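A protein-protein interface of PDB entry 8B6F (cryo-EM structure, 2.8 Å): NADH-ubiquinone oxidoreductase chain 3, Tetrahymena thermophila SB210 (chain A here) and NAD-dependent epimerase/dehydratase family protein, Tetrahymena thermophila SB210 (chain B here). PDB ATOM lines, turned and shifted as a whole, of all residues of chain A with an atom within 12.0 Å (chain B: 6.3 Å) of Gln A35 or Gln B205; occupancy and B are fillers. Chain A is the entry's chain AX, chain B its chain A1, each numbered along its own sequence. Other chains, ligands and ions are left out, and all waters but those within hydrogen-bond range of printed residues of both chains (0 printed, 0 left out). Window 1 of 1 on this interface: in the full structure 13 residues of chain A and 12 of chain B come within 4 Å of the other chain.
OE1 of Glu B85 is in salt-bridge range of NZ of Lys A34 (2.7 Å).
NE2 of Gln A36 is in hydrogen-bond range of OE2 of Glu B85.
SD of Met B204 lies within hydrogen-bond range of N of Leu A37 (3.7 Å).
The backbone carbonyl oxygen (O) of Gln A35 sits at hydrogen-bond distance from the side-chain amide nitrogen (NE2) of Gln B205, 3.0 Å away.
The side-chain carboxylate (OD2) of Asp B348 sits at hydrogen-bond distance from the side-chain amide nitrogen (NE2) of Gln A41 (3.5 Å).
The side-chain hydroxyl (OH) of Tyr B57 is in hydrogen-bond range of the side-chain amide oxygen (OE1) of Gln B205, at 2.6 Å.
The side-chain amide nitrogen (NE2) of Gln B205 sits close to the side-chain sulfur (SD) of Met B204, at 3.8 Å.
The backbone NH (N) of Arg B210 sits at hydrogen-bond distance from the side-chain carboxylate (OD1) of Asp B206, at 2.9 Å.
The side-chain amide oxygen (OE1) of Gln A35 sits at hydrogen-bond distance from the side-chain amino group (NZ) of Lys A40 (3.0 Å).
The backbone carbonyl oxygen of Leu A37 lies within hydrogen-bond range of the side-chain amide nitrogen of Gln A41, at 3.4 Å.
Among the printed residues, merely in contact across the chains: Thr A32 with Tyr B82 (3.2 Å), Gln A35 with Met B204 (3.3 Å), Lys A34 with Tyr B82 (3.5 Å), Val A33 with Tyr B82 (3.6 Å), Gln A35 with Arg B210 (3.7 Å) and Gln A36 with Met B204 (3.9 Å).
Of the printed residues of chain B, Leu A37 touches Met B204.
Of the printed residues of chain B, Gln A41 touches Asp B348 (3.5 Å).
Phe A42 touches none of the printed residues of chain B.
Tyr B57 touches none of the printed residues of chain A.
No residue of chain A comes within 4 Å of Gly B203.
Gln B205 touches just one residue of chain A: Gln A35 (3.0 Å).
No residue of chain A comes within 4 Å of Asp B206.
Arg B210 touches one residue of chain A.
The nearest residue of chain B that does not touch Gln A35 is Lys B214 (4.8 Å).
Along chain A the printed residues that touch a printed residue of chain B span positions 32 to 41.
Among the printed residues, 11 pairs touch across the chains.
Among the printed residues, Asp or Glu carboxylates within 4 Å of a Lys or Arg side-chain nitrogen of the other chain: Lys A34 with Glu B85.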
ATOM      1  N   TYR A  31      -6.369 -23.268 -17.736  1.00  0.00           N
ATOM      2  CA  TYR A  31      -5.877 -22.545 -16.569  1.00  0.00           C
ATOM      3  C   TYR A  31      -6.855 -21.428 -16.246  1.00  0.00           C
ATOM      4  O   TYR A  31      -7.593 -20.956 -17.114  1.00  0.00           O
ATOM      5  CB  TYR A  31      -4.472 -21.977 -16.791  1.00  0.00           C
ATOM      6  CG  TYR A  31      -4.381 -20.986 -17.923  1.00  0.00           C
ATOM      7  CD1 TYR A  31      -4.113 -21.406 -19.217  1.00  0.00           C
ATOM      8  CD2 TYR A  31      -4.558 -19.628 -17.698  1.00  0.00           C
ATOM      9  CE1 TYR A  31      -4.027 -20.503 -20.255  1.00  0.00           C
ATOM     10  CE2 TYR A  31      -4.473 -18.717 -18.729  1.00  0.00           C
ATOM     11  CZ  TYR A  31      -4.208 -19.162 -20.005  1.00  0.00           C
ATOM     12  OH  TYR A  31      -4.123 -18.260 -21.037  1.00  0.00           O
ATOM     13  N   THR A  32      -6.852 -21.016 -14.980  1.00  0.00           N
ATOM     14  CA  THR A  32      -7.684 -19.921 -14.504  1.00  0.00           C
ATOM     15  C   THR A  32      -6.799 -18.884 -13.831  1.00  0.00           C
ATOM     16  O   THR A  32      -5.862 -19.232 -13.106  1.00  0.00           O
ATOM     17  CB  THR A  32      -8.759 -20.416 -13.529  1.00  0.00           C
ATOM     18  OG1 THR A  32      -9.658 -19.343 -13.220  1.00  0.00           O
ATOM     19  CG2 THR A  32      -8.131 -20.924 -12.240  1.00  0.00           C
ATOM     20  N   VAL A  33      -7.099 -17.612 -14.072  1.00  0.00           N
ATOM     21  CA  VAL A  33      -6.304 -16.499 -13.567  1.00  0.00           C
ATOM     22  C   VAL A  33      -7.109 -15.816 -12.469  1.00  0.00           C
ATOM     23  O   VAL A  33      -8.163 -15.226 -12.736  1.00  0.00           O
ATOM     24  CB  VAL A  33      -5.939 -15.512 -14.684  1.00  0.00           C
ATOM     25  CG1 VAL A  33      -4.980 -14.456 -14.171  1.00  0.00           C
ATOM     26  CG2 VAL A  33      -5.335 -16.249 -15.869  1.00  0.00           C
ATOM     27  N   LYS A  34      -6.618 -15.896 -11.237  1.00  0.00           N
ATOM     28  CA  LYS A  34      -7.260 -15.219 -10.122  1.00  0.00           C
ATOM     29  C   LYS A  34      -6.858 -13.750 -10.089  1.00  0.00           C
ATOM     30  O   LYS A  34      -5.782 -13.367 -10.556  1.00  0.00           O
ATOM     31  CB  LYS A  34      -6.888 -15.893  -8.797  1.00  0.00           C
ATOM     32  CG  LYS A  34      -7.316 -15.107  -7.563  1.00  0.00           C
ATOM     33  CD  LYS A  34      -7.062 -15.874  -6.278  1.00  0.00           C
ATOM     34  CE  LYS A  34      -8.100 -16.955  -6.057  1.00  0.00           C
ATOM     35  NZ  LYS A  34      -7.960 -17.578  -4.710  1.00  0.00           N
ATOM     36  N   GLN A  35      -7.741 -12.925  -9.535  1.00  0.00           N
ATOM     37  CA  GLN A  35      -7.480 -11.501  -9.373  1.00  0.00           C
ATOM     38  C   GLN A  35      -6.743 -11.280  -8.058  1.00  0.00           C
ATOM     39  O   GLN A  35      -7.228 -11.681  -6.996  1.00  0.00           O
ATOM     40  CB  GLN A  35      -8.788 -10.708  -9.401  1.00  0.00           C
ATOM     41  CG  GLN A  35      -8.615  -9.208  -9.223  1.00  0.00           C
ATOM     42  CD  GLN A  35      -7.810  -8.573 -10.338  1.00  0.00           C
ATOM     43  OE1 GLN A  35      -7.718  -9.113 -11.439  1.00  0.00           O
ATOM     44  NE2 GLN A  35      -7.219  -7.418 -10.056  1.00  0.00           N
ATOM     45  N   GLN A  36      -5.574 -10.649  -8.132  1.00  0.00           N
ATOM     46  CA  GLN A  36      -4.763 -10.380  -6.954  1.00  0.00           C
ATOM     47  C   GLN A  36      -4.213  -8.964  -7.041  1.00  0.00           C
ATOM     48  O   GLN A  36      -4.131  -8.371  -8.119  1.00  0.00           O
ATOM     49  CB  GLN A  36      -3.632 -11.404  -6.809  1.00  0.00           C
ATOM     50  CG  GLN A  36      -4.132 -12.785  -6.417  1.00  0.00           C
ATOM     51  CD  GLN A  36      -3.060 -13.845  -6.509  1.00  0.00           C
ATOM     52  OE1 GLN A  36      -2.033 -13.651  -7.156  1.00  0.00           O
ATOM     53  NE2 GLN A  36      -3.295 -14.981  -5.862  1.00  0.00           N
ATOM     54  N   LEU A  37      -3.834  -8.429  -5.881  1.00  0.00           N
ATOM     55  CA  LEU A  37      -3.505  -7.010  -5.787  1.00  0.00           C
ATOM     56  C   LEU A  37      -2.358  -6.637  -6.716  1.00  0.00           C
ATOM     57  O   LEU A  37      -2.473  -5.704  -7.518  1.00  0.00           O
ATOM     58  CB  LEU A  37      -3.162  -6.656  -4.339  1.00  0.00           C
ATOM     59  CG  LEU A  37      -2.799  -5.196  -4.063  1.00  0.00           C
ATOM     60  CD1 LEU A  37      -3.928  -4.266  -4.473  1.00  0.00           C
ATOM     61  CD2 LEU A  37      -2.455  -5.003  -2.594  1.00  0.00           C
ATOM     62  N   THR A  38      -1.244  -7.359  -6.631  1.00  0.00           N
ATOM     63  CA  THR A  38      -0.030  -7.013  -7.355  1.00  0.00           C
ATOM     64  C   THR A  38       0.172  -7.851  -8.611  1.00  0.00           C
ATOM     65  O   THR A  38       1.256  -7.811  -9.201  1.00  0.00           O
ATOM     66  CB  THR A  38       1.187  -7.156  -6.441  1.00  0.00           C
ATOM     67  OG1 THR A  38       1.414  -8.542  -6.165  1.00  0.00           O
ATOM     68  CG2 THR A  38       0.972  -6.412  -5.131  1.00  0.00           C
ATOM     69  N   LYS A  39      -0.840  -8.607  -9.034  1.00  0.00           N
ATOM     70  CA  LYS A  39      -0.673  -9.481 -10.189  1.00  0.00           C
ATOM     71  C   LYS A  39      -0.522  -8.692 -11.482  1.00  0.00           C
ATOM     72  O   LYS A  39       0.126  -9.167 -12.420  1.00  0.00           O
ATOM     73  CB  LYS A  39      -1.857 -10.439 -10.290  1.00  0.00           C
ATOM     74  CG  LYS A  39      -1.711 -11.489 -11.375  1.00  0.00           C
ATOM     75  CD  LYS A  39      -2.699 -12.624 -11.170  1.00  0.00           C
ATOM     76  CE  LYS A  39      -2.444 -13.766 -12.134  1.00  0.00           C
ATOM     77  NZ  LYS A  39      -1.080 -14.343 -11.990  1.00  0.00           N
ATOM     78  N   LYS A  40      -1.103  -7.499 -11.554  1.00  0.00           N
ATOM     79  CA  LYS A  40      -1.087  -6.678 -12.758  1.00  0.00           C
ATOM     80  C   LYS A  40      -0.395  -5.346 -12.501  1.00  0.00           C
ATOM     81  O   LYS A  40      -0.867  -4.289 -12.920  1.00  0.00           O
ATOM     82  CB  LYS A  40      -2.504  -6.449 -13.277  1.00  0.00           C
ATOM     83  CG  LYS A  40      -3.253  -7.722 -13.629  1.00  0.00           C
ATOM     84  CD  LYS A  40      -4.644  -7.410 -14.156  1.00  0.00           C
ATOM     85  CE  LYS A  40      -5.381  -8.673 -14.570  1.00  0.00           C
ATOM     86  NZ  LYS A  40      -5.594  -9.605 -13.428  1.00  0.00           N
ATOM     87  N   GLN A  41       0.737  -5.386 -11.806  1.00  0.00           N
ATOM     88  CA  GLN A  41       1.529  -4.202 -11.515  1.00  0.00           C
ATOM     89  C   GLN A  41       2.945  -4.388 -12.045  1.00  0.00           C
ATOM     90  O   GLN A  41       3.372  -5.502 -12.360  1.00  0.00           O
ATOM     91  CB  GLN A  41       1.563  -3.911 -10.011  1.00  0.00           C
ATOM     92  CG  GLN A  41       0.198  -3.576  -9.428  1.00  0.00           C
ATOM     93  CD  GLN A  41       0.268  -3.176  -7.970  1.00  0.00           C
ATOM     94  OE1 GLN A  41       1.325  -3.245  -7.344  1.00  0.00           O
ATOM     95  NE2 GLN A  41      -0.863  -2.749  -7.421  1.00  0.00           N
ATOM     96  N   PHE A  42       3.670  -3.279 -12.143  1.00  0.00           N
ATOM     97  CA  PHE A  42       5.013  -3.316 -12.702  1.00  0.00           C
ATOM     98  C   PHE A  42       5.940  -4.149 -11.824  1.00  0.00           C
ATOM     99  O   PHE A  42       5.890  -4.077 -10.593  1.00  0.00           O
ATOM    100  CB  PHE A  42       5.565  -1.900 -12.854  1.00  0.00           C
ATOM    101  CG  PHE A  42       4.741  -1.025 -13.749  1.00  0.00           C
ATOM    102  CD1 PHE A  42       4.548  -1.359 -15.078  1.00  0.00           C
ATOM    103  CD2 PHE A  42       4.173   0.142 -13.266  1.00  0.00           C
ATOM    104  CE1 PHE A  42       3.793  -0.554 -15.906  1.00  0.00           C
ATOM    105  CE2 PHE A  42       3.418   0.952 -14.087  1.00  0.00           C
ATOM    106  CZ  PHE A  42       3.228   0.604 -15.410  1.00  0.00           C
ATOM    107  N   PHE B  53     -15.833 -17.472  -5.039  1.00  0.00           N
ATOM    108  CA  PHE B  53     -15.293 -16.150  -4.735  1.00  0.00           C
ATOM    109  C   PHE B  53     -15.311 -15.878  -3.238  1.00  0.00           C
ATOM    110  O   PHE B  53     -14.345 -15.338  -2.685  1.00  0.00           O
ATOM    111  CB  PHE B  53     -16.084 -15.077  -5.484  1.00  0.00           C
ATOM    112  CG  PHE B  53     -16.172 -13.765  -4.757  1.00  0.00           C
ATOM    113  CD1 PHE B  53     -15.040 -12.998  -4.543  1.00  0.00           C
ATOM    114  CD2 PHE B  53     -17.392 -13.285  -4.312  1.00  0.00           C
ATOM    115  CE1 PHE B  53     -15.118 -11.788  -3.883  1.00  0.00           C
ATOM    116  CE2 PHE B  53     -17.477 -12.075  -3.651  1.00  0.00           C
ATOM    117  CZ  PHE B  53     -16.338 -11.325  -3.440  1.00  0.00           C
ATOM    118  N   TYR B  57     -12.703 -16.055   1.752  1.00  0.00           N
ATOM    119  CA  TYR B  57     -12.952 -15.029   2.759  1.00  0.00           C
ATOM    120  C   TYR B  57     -13.682 -15.604   3.967  1.00  0.00           C
ATOM    121  O   TYR B  57     -13.304 -15.343   5.115  1.00  0.00           O
ATOM    122  CB  TYR B  57     -13.753 -13.883   2.143  1.00  0.00           C
ATOM    123  CG  TYR B  57     -12.955 -13.025   1.194  1.00  0.00           C
ATOM    124  CD1 TYR B  57     -12.799 -13.382  -0.137  1.00  0.00           C
ATOM    125  CD2 TYR B  57     -12.362 -11.850   1.631  1.00  0.00           C
ATOM    126  CE1 TYR B  57     -12.072 -12.595  -1.006  1.00  0.00           C
ATOM    127  CE2 TYR B  57     -11.635 -11.056   0.771  1.00  0.00           C
ATOM    128  CZ  TYR B  57     -11.493 -11.433  -0.546  1.00  0.00           C
ATOM    129  OH  TYR B  57     -10.766 -10.642  -1.402  1.00  0.00           O
ATOM    130  N   TYR B  82      -7.656 -20.873  -6.748  1.00  0.00           N
ATOM    131  CA  TYR B  82      -8.838 -20.891  -5.896  1.00  0.00           C
ATOM    132  C   TYR B  82      -8.761 -22.016  -4.873  1.00  0.00           C
ATOM    133  O   TYR B  82      -9.074 -21.817  -3.694  1.00  0.00           O
ATOM    134  CB  TYR B  82     -10.095 -21.029  -6.754  1.00  0.00           C
ATOM    135  CG  TYR B  82     -10.231 -19.945  -7.795  1.00  0.00           C
ATOM    136  CD1 TYR B  82     -10.767 -18.706  -7.472  1.00  0.00           C
ATOM    137  CD2 TYR B  82      -9.820 -20.160  -9.102  1.00  0.00           C
ATOM    138  CE1 TYR B  82     -10.889 -17.711  -8.421  1.00  0.00           C
ATOM    139  CE2 TYR B  82      -9.939 -19.173 -10.058  1.00  0.00           C
ATOM    140  CZ  TYR B  82     -10.474 -17.951  -9.714  1.00  0.00           C
ATOM    141  OH  TYR B  82     -10.591 -16.967 -10.668  1.00  0.00           O
ATOM    142  N   GLU B  85      -5.222 -21.385  -2.454  1.00  0.00           N
ATOM    143  CA  GLU B  85      -5.176 -20.353  -1.427  1.00  0.00           C
ATOM    144  C   GLU B  85      -6.033 -20.679  -0.212  1.00  0.00           C
ATOM    145  O   GLU B  85      -5.918 -19.987   0.804  1.00  0.00           O
ATOM    146  CB  GLU B  85      -5.606 -19.008  -2.015  1.00  0.00           C
ATOM    147  CG  GLU B  85      -4.577 -18.402  -2.955  1.00  0.00           C
ATOM    148  CD  GLU B  85      -4.907 -16.974  -3.342  1.00  0.00           C
ATOM    149  OE1 GLU B  85      -6.038 -16.525  -3.059  1.00  0.00           O
ATOM    150  OE2 GLU B  85      -4.034 -16.298  -3.927  1.00  0.00           O
ATOM    151  N   GLY B 203     -16.071  -7.160  -4.360  1.00  0.00           N
ATOM    152  CA  GLY B 203     -14.760  -7.329  -3.769  1.00  0.00           C
ATOM    153  C   GLY B 203     -13.718  -7.466  -4.857  1.00  0.00           C
ATOM    154  O   GLY B 203     -14.003  -7.275  -6.040  1.00  0.00           O
ATOM    155  N   MET B 204     -12.495  -7.802  -4.441  1.00  0.00           N
ATOM    156  CA  MET B 204     -11.402  -7.895  -5.403  1.00  0.00           C
ATOM    157  C   MET B 204     -11.640  -9.013  -6.411  1.00  0.00           C
ATOM    158  O   MET B 204     -11.420  -8.830  -7.613  1.00  0.00           O
ATOM    159  CB  MET B 204     -10.077  -8.102  -4.671  1.00  0.00           C
ATOM    160  CG  MET B 204      -8.871  -8.160  -5.600  1.00  0.00           C
ATOM    161  SD  MET B 204      -7.293  -8.117  -4.730  1.00  0.00           S
ATOM    162  CE  MET B 204      -7.294  -6.445  -4.091  1.00  0.00           C
ATOM    163  N   GLN B 205     -12.092 -10.177  -5.945  1.00  0.00           N
ATOM    164  CA  GLN B 205     -12.331 -11.329  -6.804  1.00  0.00           C
ATOM    165  C   GLN B 205     -13.813 -11.544  -7.088  1.00  0.00           C
ATOM    166  O   GLN B 205     -14.216 -12.657  -7.440  1.00  0.00           O
ATOM    167  CB  GLN B 205     -11.732 -12.593  -6.182  1.00  0.00           C
ATOM    168  CG  GLN B 205     -10.236 -12.525  -5.919  1.00  0.00           C
ATOM    169  CD  GLN B 205      -9.896 -11.784  -4.644  1.00  0.00           C
ATOM    170  OE1 GLN B 205     -10.779 -11.367  -3.900  1.00  0.00           O
ATOM    171  NE2 GLN B 205      -8.605 -11.619  -4.385  1.00  0.00           N
ATOM    172  N   ASP B 206     -14.629 -10.504  -6.943  1.00  0.00           N
ATOM    173  CA  ASP B 206     -16.068 -10.645  -7.091  1.00  0.00           C
ATOM    174  C   ASP B 206     -16.436 -10.909  -8.548  1.00  0.00           C
ATOM    175  O   ASP B 206     -15.584 -10.980  -9.438  1.00  0.00           O
ATOM    176  CB  ASP B 206     -16.775  -9.390  -6.592  1.00  0.00           C
ATOM    177  CG  ASP B 206     -16.429  -8.164  -7.416  1.00  0.00           C
ATOM    178  OD1 ASP B 206     -15.497  -8.243  -8.241  1.00  0.00           O
ATOM    179  OD2 ASP B 206     -17.090  -7.119  -7.243  1.00  0.00           O
ATOM    180  N   TYR B 207     -17.736 -11.060  -8.784  1.00  0.00           N
ATOM    181  CA  TYR B 207     -18.291 -11.188 -10.122  1.00  0.00           C
ATOM    182  C   TYR B 207     -18.984  -9.914 -10.584  1.00  0.00           C
ATOM    183  O   TYR B 207     -19.659  -9.931 -11.617  1.00  0.00           O
ATOM    184  CB  TYR B 207     -19.281 -12.353 -10.176  1.00  0.00           C
ATOM    185  CG  TYR B 207     -18.676 -13.695  -9.840  1.00  0.00           C
ATOM    186  CD1 TYR B 207     -17.912 -14.386 -10.769  1.00  0.00           C
ATOM    187  CD2 TYR B 207     -18.887 -14.278  -8.600  1.00  0.00           C
ATOM    188  CE1 TYR B 207     -17.363 -15.616 -10.467  1.00  0.00           C
ATOM    189  CE2 TYR B 207     -18.344 -15.505  -8.287  1.00  0.00           C
ATOM    190  CZ  TYR B 207     -17.584 -16.170  -9.224  1.00  0.00           C
ATOM    191  OH  TYR B 207     -17.042 -17.395  -8.915  1.00  0.00           O
ATOM    192  N   ARG B 210     -15.157  -6.754 -10.743  1.00  0.00           N
ATOM    193  CA  ARG B 210     -14.198  -7.351 -11.662  1.00  0.00           C
ATOM    194  C   ARG B 210     -14.825  -7.592 -13.028  1.00  0.00           C
ATOM    195  O   ARG B 210     -14.186  -7.362 -14.061  1.00  0.00           O
ATOM    196  CB  ARG B 210     -13.661  -8.658 -11.077  1.00  0.00           C
ATOM    197  CG  ARG B 210     -12.637  -9.359 -11.956  1.00  0.00           C
ATOM    198  CD  ARG B 210     -12.029 -10.557 -11.246  1.00  0.00           C
ATOM    199  NE  ARG B 210     -13.042 -11.526 -10.845  1.00  0.00           N
ATOM    200  CZ  ARG B 210     -13.534 -12.470 -11.635  1.00  0.00           C
ATOM    201  NH1 ARG B 210     -13.133 -12.601 -12.888  1.00  0.00           N
ATOM    202  NH2 ARG B 210     -14.449 -13.306 -11.154  1.00  0.00           N
ATOM    203  N   LYS B 214     -13.494  -5.961 -16.453  1.00  0.00           N
ATOM    204  CA  LYS B 214     -13.024  -6.834 -17.523  1.00  0.00           C
ATOM    205  C   LYS B 214     -13.852  -6.666 -18.788  1.00  0.00           C
ATOM    206  O   LYS B 214     -13.307  -6.674 -19.897  1.00  0.00           O
ATOM    207  CB  LYS B 214     -13.035  -8.291 -17.066  1.00  0.00           C
ATOM    208  CG  LYS B 214     -11.924  -8.633 -16.086  1.00  0.00           C
ATOM    209  CD  LYS B 214     -11.814 -10.134 -15.871  1.00  0.00           C
ATOM    210  CE  LYS B 214     -10.656 -10.472 -14.946  1.00  0.00           C
ATOM    211  NZ  LYS B 214     -10.449 -11.941 -14.815  1.00  0.00           N
ATOM    212  N   PHE B 345     -10.902  -0.812  -4.927  1.00  0.00           N
ATOM    213  CA  PHE B 345     -10.749  -1.902  -5.882  1.00  0.00           C
ATOM    214  C   PHE B 345     -10.630  -1.426  -7.322  1.00  0.00           C
ATOM    215  O   PHE B 345     -10.493  -2.263  -8.220  1.00  0.00           O
ATOM    216  CB  PHE B 345     -11.928  -2.869  -5.756  1.00  0.00           C
ATOM    217  CG  PHE B 345     -12.111  -3.414  -4.372  1.00  0.00           C
ATOM    218  CD1 PHE B 345     -11.276  -4.406  -3.889  1.00  0.00           C
ATOM    219  CD2 PHE B 345     -13.118  -2.935  -3.552  1.00  0.00           C
ATOM    220  CE1 PHE B 345     -11.440  -4.909  -2.614  1.00  0.00           C
ATOM    221  CE2 PHE B 345     -13.289  -3.435  -2.276  1.00  0.00           C
ATOM    222  CZ  PHE B 345     -12.448  -4.423  -1.806  1.00  0.00           C
ATOM    223  N   ASP B 348      -6.172   0.886  -9.556  1.00  0.00           N
ATOM    224  CA  ASP B 348      -5.320   0.604 -10.706  1.00  0.00           C
ATOM    225  C   ASP B 348      -5.998   1.013 -12.006  1.00  0.00           C
ATOM    226  O   ASP B 348      -5.361   1.600 -12.888  1.00  0.00           O
ATOM    227  CB  ASP B 348      -4.950  -0.878 -10.740  1.00  0.00           C
ATOM    228  CG  ASP B 348      -3.923  -1.249  -9.686  1.00  0.00           C
ATOM    229  OD1 ASP B 348      -3.419  -0.336  -8.997  1.00  0.00           O
ATOM    230  OD2 ASP B 348      -3.618  -2.452  -9.549  1.00  0.00           O
